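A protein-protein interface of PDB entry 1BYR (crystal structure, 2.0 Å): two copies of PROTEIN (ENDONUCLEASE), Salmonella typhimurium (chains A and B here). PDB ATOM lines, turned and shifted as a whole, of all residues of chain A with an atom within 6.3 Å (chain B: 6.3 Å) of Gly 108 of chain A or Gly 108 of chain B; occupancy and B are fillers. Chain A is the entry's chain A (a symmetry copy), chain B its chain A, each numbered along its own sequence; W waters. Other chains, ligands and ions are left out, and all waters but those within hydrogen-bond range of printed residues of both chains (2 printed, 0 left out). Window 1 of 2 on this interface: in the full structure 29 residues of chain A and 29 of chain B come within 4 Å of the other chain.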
ATOM      1  N   LYS A  96       9.567  10.763  23.673  1.00  0.00           N
ATOM      2  CA  LYS A  96       8.109  10.912  23.656  1.00  0.00           C
ATOM      3  C   LYS A  96       7.806  10.656  25.133  1.00  0.00           C
ATOM      4  O   LYS A  96       7.485   9.540  25.548  1.00  0.00           O
ATOM      5  CB  LYS A  96       7.443   9.844  22.765  1.00  0.00           C
ATOM      6  CG  LYS A  96       8.042   9.737  21.369  1.00  0.00           C
ATOM      7  CD  LYS A  96       9.129   8.634  21.322  1.00  0.00           C
ATOM      8  CE  LYS A  96       9.366   8.096  19.911  1.00  0.00           C
ATOM      9  NZ  LYS A  96       9.753   9.182  18.969  1.00  0.00           N
ATOM     10  N   VAL A  97       7.933  11.712  25.920  1.00  0.00           N
ATOM     11  CA  VAL A  97       7.777  11.612  27.362  1.00  0.00           C
ATOM     12  C   VAL A  97       6.866  12.665  27.993  1.00  0.00           C
ATOM     13  O   VAL A  97       6.879  13.832  27.601  1.00  0.00           O
ATOM     14  CB  VAL A  97       9.169  11.748  28.037  1.00  0.00           C
ATOM     15  CG1 VAL A  97       9.016  11.929  29.560  1.00  0.00           C
ATOM     16  CG2 VAL A  97      10.044  10.542  27.699  1.00  0.00           C
ATOM     17  N   GLU A 106       5.202   9.000  31.719  1.00  0.00           N
ATOM     18  CA  GLU A 106       4.635   8.274  30.596  1.00  0.00           C
ATOM     19  C   GLU A 106       5.787   8.222  29.602  1.00  0.00           C
ATOM     20  O   GLU A 106       6.508   9.211  29.451  1.00  0.00           O
ATOM     21  CB  GLU A 106       3.474   9.063  29.954  1.00  0.00           C
ATOM     22  CG  GLU A 106       2.829   8.386  28.735  1.00  0.00           C
ATOM     23  CD  GLU A 106       3.583   8.633  27.437  1.00  0.00           C
ATOM     24  OE1 GLU A 106       4.201   9.706  27.295  1.00  0.00           O
ATOM     25  OE2 GLU A 106       3.557   7.746  26.554  1.00  0.00           O
ATOM     26  N   THR A 107       5.987   7.077  28.948  1.00  0.00           N
ATOM     27  CA  THR A 107       7.042   6.965  27.943  1.00  0.00           C
ATOM     28  C   THR A 107       6.761   5.749  27.084  1.00  0.00           C
ATOM     29  O   THR A 107       5.774   5.049  27.310  1.00  0.00           O
ATOM     30  CB  THR A 107       8.456   6.869  28.557  1.00  0.00           C
ATOM     31  OG1 THR A 107       9.420   7.014  27.508  1.00  0.00           O
ATOM     32  CG2 THR A 107       8.668   5.515  29.253  1.00  0.00           C
ATOM     33  N   GLY A 108       7.603   5.502  26.081  1.00  0.00           N
ATOM     34  CA  GLY A 108       7.388   4.371  25.192  1.00  0.00           C
ATOM     35  C   GLY A 108       7.724   4.738  23.757  1.00  0.00           C
ATOM     36  O   GLY A 108       8.512   5.644  23.519  1.00  0.00           O
ATOM     37  N   SER A 109       7.143   4.033  22.788  1.00  0.00           N
ATOM     38  CA  SER A 109       7.422   4.340  21.388  1.00  0.00           C
ATOM     39  C   SER A 109       6.459   5.390  20.839  1.00  0.00           C
ATOM     40  O   SER A 109       6.778   6.102  19.887  1.00  0.00           O
ATOM     41  CB  SER A 109       7.313   3.078  20.526  1.00  0.00           C
ATOM     42  OG  SER A 109       5.963   2.689  20.329  1.00  0.00           O
ATOM     43  N   PHE A 110       5.287   5.465  21.459  1.00  0.00           N
ATOM     44  CA  PHE A 110       4.190   6.357  21.064  1.00  0.00           C
ATOM     45  C   PHE A 110       4.508   7.849  20.842  1.00  0.00           C
ATOM     46  O   PHE A 110       4.809   8.583  21.797  1.00  0.00           O
ATOM     47  CB  PHE A 110       3.060   6.192  22.103  1.00  0.00           C
ATOM     48  CG  PHE A 110       1.784   6.959  21.794  1.00  0.00           C
ATOM     49  CD1 PHE A 110       1.615   8.271  22.230  1.00  0.00           C
ATOM     50  CD2 PHE A 110       0.716   6.333  21.174  1.00  0.00           C
ATOM     51  CE1 PHE A 110       0.392   8.933  22.051  1.00  0.00           C
ATOM     52  CE2 PHE A 110      -0.511   7.001  20.996  1.00  0.00           C
ATOM     53  CZ  PHE A 110      -0.667   8.288  21.435  1.00  0.00           C
ATOM     54  N   ASN A 111       4.451   8.295  19.585  1.00  0.00           N
ATOM     55  CA  ASN A 111       4.681   9.713  19.272  1.00  0.00           C
ATOM     56  C   ASN A 111       3.326  10.378  19.423  1.00  0.00           C
ATOM     57  O   ASN A 111       2.290   9.730  19.288  1.00  0.00           O
ATOM     58  CB  ASN A 111       5.149   9.930  17.837  1.00  0.00           C
ATOM     59  CG  ASN A 111       6.616   9.698  17.667  1.00  0.00           C
ATOM     60  OD1 ASN A 111       7.032   8.714  17.058  1.00  0.00           O
ATOM     61  ND2 ASN A 111       7.420  10.585  18.198  1.00  0.00           N
ATOM     62  N   GLU A 122       2.372   0.459  18.403  1.00  0.00           N
ATOM     63  CA  GLU A 122       3.101   1.228  19.407  1.00  0.00           C
ATOM     64  C   GLU A 122       2.757   0.708  20.777  1.00  0.00           C
ATOM     65  O   GLU A 122       1.833  -0.077  20.952  1.00  0.00           O
ATOM     66  CB  GLU A 122       2.689   2.717  19.415  1.00  0.00           C
ATOM     67  CG  GLU A 122       2.552   3.392  18.082  1.00  0.00           C
ATOM     68  CD  GLU A 122       3.824   4.058  17.636  1.00  0.00           C
ATOM     69  OE1 GLU A 122       4.859   3.872  18.301  1.00  0.00           O
ATOM     70  OE2 GLU A 122       3.783   4.771  16.616  1.00  0.00           O
ATOM     71  N   ASN A 123       3.519   1.172  21.759  1.00  0.00           N
ATOM     72  CA  ASN A 123       3.249   0.848  23.144  1.00  0.00           C
ATOM     73  C   ASN A 123       3.512   2.126  23.922  1.00  0.00           C
ATOM     74  O   ASN A 123       4.405   2.906  23.580  1.00  0.00           O
ATOM     75  CB  ASN A 123       4.160  -0.279  23.657  1.00  0.00           C
ATOM     76  CG  ASN A 123       5.605   0.153  23.811  1.00  0.00           C
ATOM     77  OD1 ASN A 123       6.371   0.148  22.848  1.00  0.00           O
ATOM     78  ND2 ASN A 123       5.982   0.542  25.011  1.00  0.00           N
ATOM     79  N   ALA A 124       2.692   2.376  24.938  1.00  0.00           N
ATOM     80  CA  ALA A 124       2.884   3.512  25.815  1.00  0.00           C
ATOM     81  C   ALA A 124       2.741   2.968  27.214  1.00  0.00           C
ATOM     82  O   ALA A 124       1.845   2.160  27.478  1.00  0.00           O
ATOM     83  CB  ALA A 124       1.802   4.611  25.562  1.00  0.00           C
ATOM     84  N   VAL A 125       3.639   3.376  28.109  1.00  0.00           N
ATOM     85  CA  VAL A 125       3.545   2.946  29.489  1.00  0.00           C
ATOM     86  C   VAL A 125       3.474   4.163  30.394  1.00  0.00           C
ATOM     87  O   VAL A 125       4.033   5.225  30.085  1.00  0.00           O
ATOM     88  CB  VAL A 125       4.767   2.084  29.918  1.00  0.00           C
ATOM     89  CG1 VAL A 125       4.820   0.819  29.080  1.00  0.00           C
ATOM     90  CG2 VAL A 125       6.054   2.884  29.779  1.00  0.00           C
ATOM     91  N   LYS B  96       9.913  -0.472  20.206  1.00  0.00           N
ATOM     92  CA  LYS B  96      11.333  -0.702  20.481  1.00  0.00           C
ATOM     93  C   LYS B  96      11.228  -1.342  21.866  1.00  0.00           C
ATOM     94  O   LYS B  96      11.342  -0.679  22.901  1.00  0.00           O
ATOM     95  CB  LYS B  96      12.117   0.624  20.547  1.00  0.00           C
ATOM     96  CG  LYS B  96      11.888   1.542  19.353  1.00  0.00           C
ATOM     97  CD  LYS B  96      10.764   2.565  19.656  1.00  0.00           C
ATOM     98  CE  LYS B  96      10.852   3.817  18.784  1.00  0.00           C
ATOM     99  NZ  LYS B  96      10.807   3.479  17.335  1.00  0.00           N
ATOM    100  N   VAL B  97      10.989  -2.643  21.863  1.00  0.00           N
ATOM    101  CA  VAL B  97      10.764  -3.380  23.097  1.00  0.00           C
ATOM    102  C   VAL B  97      11.565  -4.674  23.237  1.00  0.00           C
ATOM    103  O   VAL B  97      11.746  -5.417  22.271  1.00  0.00           O
ATOM    104  CB  VAL B  97       9.261  -3.759  23.198  1.00  0.00           C
ATOM    105  CG1 VAL B  97       9.035  -4.772  24.336  1.00  0.00           C
ATOM    106  CG2 VAL B  97       8.408  -2.505  23.383  1.00  0.00           C
ATOM    107  N   GLU B 106      11.925  -3.870  28.650  1.00  0.00           N
ATOM    108  CA  GLU B 106      12.701  -2.687  28.316  1.00  0.00           C
ATOM    109  C   GLU B 106      11.840  -1.996  27.267  1.00  0.00           C
ATOM    110  O   GLU B 106      11.262  -2.670  26.411  1.00  0.00           O
ATOM    111  CB  GLU B 106      14.046  -3.071  27.664  1.00  0.00           C
ATOM    112  CG  GLU B 106      14.925  -1.882  27.246  1.00  0.00           C
ATOM    113  CD  GLU B 106      14.549  -1.299  25.892  1.00  0.00           C
ATOM    114  OE1 GLU B 106      14.075  -2.056  25.023  1.00  0.00           O
ATOM    115  OE2 GLU B 106      14.728  -0.076  25.699  1.00  0.00           O
ATOM    116  N   THR B 107      11.723  -0.670  27.341  1.00  0.00           N
ATOM    117  CA  THR B 107      10.953   0.069  26.342  1.00  0.00           C
ATOM    118  C   THR B 107      11.346   1.531  26.418  1.00  0.00           C
ATOM    119  O   THR B 107      12.184   1.903  27.239  1.00  0.00           O
ATOM    120  CB  THR B 107       9.426  -0.082  26.520  1.00  0.00           C
ATOM    121  OG1 THR B 107       8.776   0.462  25.365  1.00  0.00           O
ATOM    122  CG2 THR B 107       8.937   0.662  27.773  1.00  0.00           C
ATOM    123  N   GLY B 108      10.771   2.363  25.550  1.00  0.00           N
ATOM    124  CA  GLY B 108      11.115   3.776  25.537  1.00  0.00           C
ATOM    125  C   GLY B 108      11.186   4.304  24.115  1.00  0.00           C
ATOM    126  O   GLY B 108      10.559   3.752  23.219  1.00  0.00           O
ATOM    127  N   SER B 109      11.937   5.381  23.893  1.00  0.00           N
ATOM    128  CA  SER B 109      12.049   5.934  22.546  1.00  0.00           C
ATOM    129  C   SER B 109      13.201   5.298  21.771  1.00  0.00           C
ATOM    130  O   SER B 109      13.194   5.269  20.541  1.00  0.00           O
ATOM    131  CB  SER B 109      12.273   7.448  22.600  1.00  0.00           C
ATOM    132  OG  SER B 109      13.593   7.771  23.007  1.00  0.00           O
ATOM    133  N   PHE B 110      14.178   4.795  22.518  1.00  0.00           N
ATOM    134  CA  PHE B 110      15.408   4.193  21.987  1.00  0.00           C
ATOM    135  C   PHE B 110      15.276   3.112  20.895  1.00  0.00           C
ATOM    136  O   PHE B 110      14.801   1.996  21.161  1.00  0.00           O
ATOM    137  CB  PHE B 110      16.218   3.658  23.187  1.00  0.00           C
ATOM    138  CG  PHE B 110      17.587   3.096  22.839  1.00  0.00           C
ATOM    139  CD1 PHE B 110      17.744   1.757  22.491  1.00  0.00           C
ATOM    140  CD2 PHE B 110      18.725   3.874  22.973  1.00  0.00           C
ATOM    141  CE1 PHE B 110      19.021   1.213  22.291  1.00  0.00           C
ATOM    142  CE2 PHE B 110      20.006   3.325  22.771  1.00  0.00           C
ATOM    143  CZ  PHE B 110      20.147   2.006  22.437  1.00  0.00           C
ATOM    144  N   ASN B 111      15.688   3.444  19.669  1.00  0.00           N
ATOM    145  CA  ASN B 111      15.660   2.466  18.570  1.00  0.00           C
ATOM    146  C   ASN B 111      16.979   1.726  18.662  1.00  0.00           C
ATOM    147  O   ASN B 111      17.960   2.254  19.183  1.00  0.00           O
ATOM    148  CB  ASN B 111      15.591   3.128  17.197  1.00  0.00           C
ATOM    149  CG  ASN B 111      14.203   3.532  16.819  1.00  0.00           C
ATOM    150  OD1 ASN B 111      13.878   4.718  16.784  1.00  0.00           O
ATOM    151  ND2 ASN B 111      13.363   2.567  16.537  1.00  0.00           N
ATOM    152  N   GLU B 122      17.367  10.403  23.653  1.00  0.00           N
ATOM    153  CA  GLU B 122      16.470   9.264  23.828  1.00  0.00           C
ATOM    154  C   GLU B 122      16.411   8.899  25.287  1.00  0.00           C
ATOM    155  O   GLU B 122      17.193   9.375  26.100  1.00  0.00           O
ATOM    156  CB  GLU B 122      16.984   7.999  23.106  1.00  0.00           C
ATOM    157  CG  GLU B 122      17.510   8.177  21.712  1.00  0.00           C
ATOM    158  CD  GLU B 122      16.451   7.978  20.664  1.00  0.00           C
ATOM    159  OE1 GLU B 122      15.269   7.842  21.028  1.00  0.00           O
ATOM    160  OE2 GLU B 122      16.808   7.958  19.471  1.00  0.00           O
ATOM    161  N   ASN B 123      15.463   8.027  25.608  1.00  0.00           N
ATOM    162  CA  ASN B 123      15.344   7.498  26.950  1.00  0.00           C
ATOM    163  C   ASN B 123      14.994   6.030  26.781  1.00  0.00           C
ATOM    164  O   ASN B 123      14.284   5.648  25.847  1.00  0.00           O
ATOM    165  CB  ASN B 123      14.245   8.213  27.752  1.00  0.00           C
ATOM    166  CG  ASN B 123      12.848   7.886  27.263  1.00  0.00           C
ATOM    167  OD1 ASN B 123      12.355   8.490  26.312  1.00  0.00           O
ATOM    168  ND2 ASN B 123      12.210   6.924  27.896  1.00  0.00           N
ATOM    169  N   ALA B 124      15.545   5.189  27.651  1.00  0.00           N
ATOM    170  CA  ALA B 124      15.227   3.776  27.657  1.00  0.00           C
ATOM    171  C   ALA B 124      14.965   3.431  29.102  1.00  0.00           C
ATOM    172  O   ALA B 124      15.696   3.878  29.991  1.00  0.00           O
ATOM    173  CB  ALA B 124      16.422   2.925  27.120  1.00  0.00           C
ATOM    174  N   VAL B 125      13.904   2.665  29.351  1.00  0.00           N
ATOM    175  CA  VAL B 125      13.608   2.240  30.703  1.00  0.00           C
ATOM    176  C   VAL B 125      13.543   0.724  30.753  1.00  0.00           C
ATOM    177  O   VAL B 125      13.168   0.065  29.773  1.00  0.00           O
ATOM    178  CB  VAL B 125      12.252   2.809  31.212  1.00  0.00           C
ATOM    179  CG1 VAL B 125      12.314   4.325  31.246  1.00  0.00           C
ATOM    180  CG2 VAL B 125      11.111   2.329  30.327  1.00  0.00           C
HETATM  181  O   HOH W   1       9.930   8.029  24.768  1.00  0.00           O
HETATM  182  O   HOH W   2       9.065   1.199  22.507  1.00  0.00           O
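The side-chain hydroxyl (OG1) of Thr 107 of chain B is in hydrogen-bond range of the side-chain amide nitrogen (ND2) of Asn 123 of chain A (2.8 Å). O of Gly 108 of chain B is in hydrogen-bond range of N of Ser 109 of chain A (3.5 Å). N of Ser 109 of chain B is in hydrogen-bond range of O of Gly 108 of chain A. ND2 of Asn 123 of chain B lies within hydrogen-bond range of OG1 of Thr 107 of chain A (2.8 Å). The backbone carbonyl oxygen of Gly 108 of chain A lies close to the backbone carbonyl oxygen of Gly 108 of chain B (2.8 Å).
NZ of Lys 96 of chain B lies close to ND2 of Asn 111 of chain B. The backbone NH (N) of Val 125 of chain B sits at hydrogen-bond distance from the backbone carbonyl oxygen (O) of Thr 107 of chain B, 2.8 Å away. OG of Ser 109 of chain B sits at hydrogen-bond distance from OE1 of Glu 122 of chain B (2.6 Å). O of Asn 123 of chain B lies within hydrogen-bond range of N of Ser 109 of chain B, 3.1 Å away. O of Thr 107 of chain A is in hydrogen-bond range of N of Val 125 of chain A (2.8 Å). The side-chain hydroxyl (OG) of Ser 109 of chain A is in hydrogen-bond range of the side-chain carboxylate (OE1) of Glu 122 of chain A, at 2.6 Å.
Lys 96 of chain A touches Ser 109 of chain B (CD to CB, 3.6 Å). Asn 123 of chain B touches Val 97 of chain A. Ser 109 of chain A touches Lys 96 of chain B. Asn 123 of chain A touches Val 97 of chain B.
Gly 108 of chain A touches just these residues of chain B: Gly 108 (2.8 Å) and Ser 109 (3.5 Å). Gly 108 of chain B touches just these residues of chain A: Gly 108 and Ser 109. Of the printed residues of chain A, Thr 107 of chain B touches Asn 123 (2.8 Å). Printed residues of chain A within 4 Å of Asn 123 of chain B: Val 97 and Thr 107. Of the printed residues of chain B, Thr 107 of chain A touches Asn 123. The nearest residue of chain B that does not touch Gly 108 of chain A is Thr 107 of chain B (4.2 Å). The nearest residue of chain A that does not touch Gly 108 of chain B is Thr 107 of chain A (4.2 Å). The nearest printed residue of chain B that does not touch Ser 109 of chain A is Thr 107 of chain B (4.7 Å).
Hydrophobic or aromatic side chains of chain B that line the printed part of chain A: Val 97. Of the 12 printed residues of chain A, 6 touch a printed residue of chain B. Among the printed residues, 9 pairs touch across the chains. Among the printed residues, no Asp or Glu carboxylate lies within 4 Å of a Lys or Arg side-chain nitrogen of the other chain.
Lys 96 of chain A touches Ser 109 of chain B, and with the chains exchanged Ser 109 of chain A touches Lys 96 of chain B. Val 97 of chain A touches Asn 123 of chain B, and with the chains exchanged Asn 123 of chain A touches Val 97 of chain B. Thr 107 of chain A touches Asn 123 of chain B, and with the chains exchanged Asn 123 of chain A touches Thr 107 of chain B. Gly 108 of chain A touches Ser 109 of chain B, and with the chains exchanged Ser 109 of chain A touches Gly 108 of chain B. 12 positions are printed for both chains. Of the 9 pairs that touch across the chains among the printed residues, 9 have their exchanged pair printed and touching as well.
Water W2 lies within hydrogen-bond range of OD1 of Asn 123 of chain A (2.9 Å), OG1 of Thr 107 of chain B (3.0 Å), N of Lys 96 of chain B (3.0 Å), O of Gly 108 of chain B (3.0 Å) and N of Ser 109 of chain A (3.4 Å). Water W1 lies within hydrogen-bond range of the side-chain amide oxygen (OD1) of Asn 123 of chain B (2.9 Å), the side-chain hydroxyl (OG1) of Thr 107 of chain A (3.0 Å), the backbone NH (N) of Lys 96 of chain A (3.0 Å), the backbone carbonyl oxygen (O) of Gly 108 of chain A (3.0 Å) and the backbone NH (N) of Ser 109 of chain B (3.4 Å).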
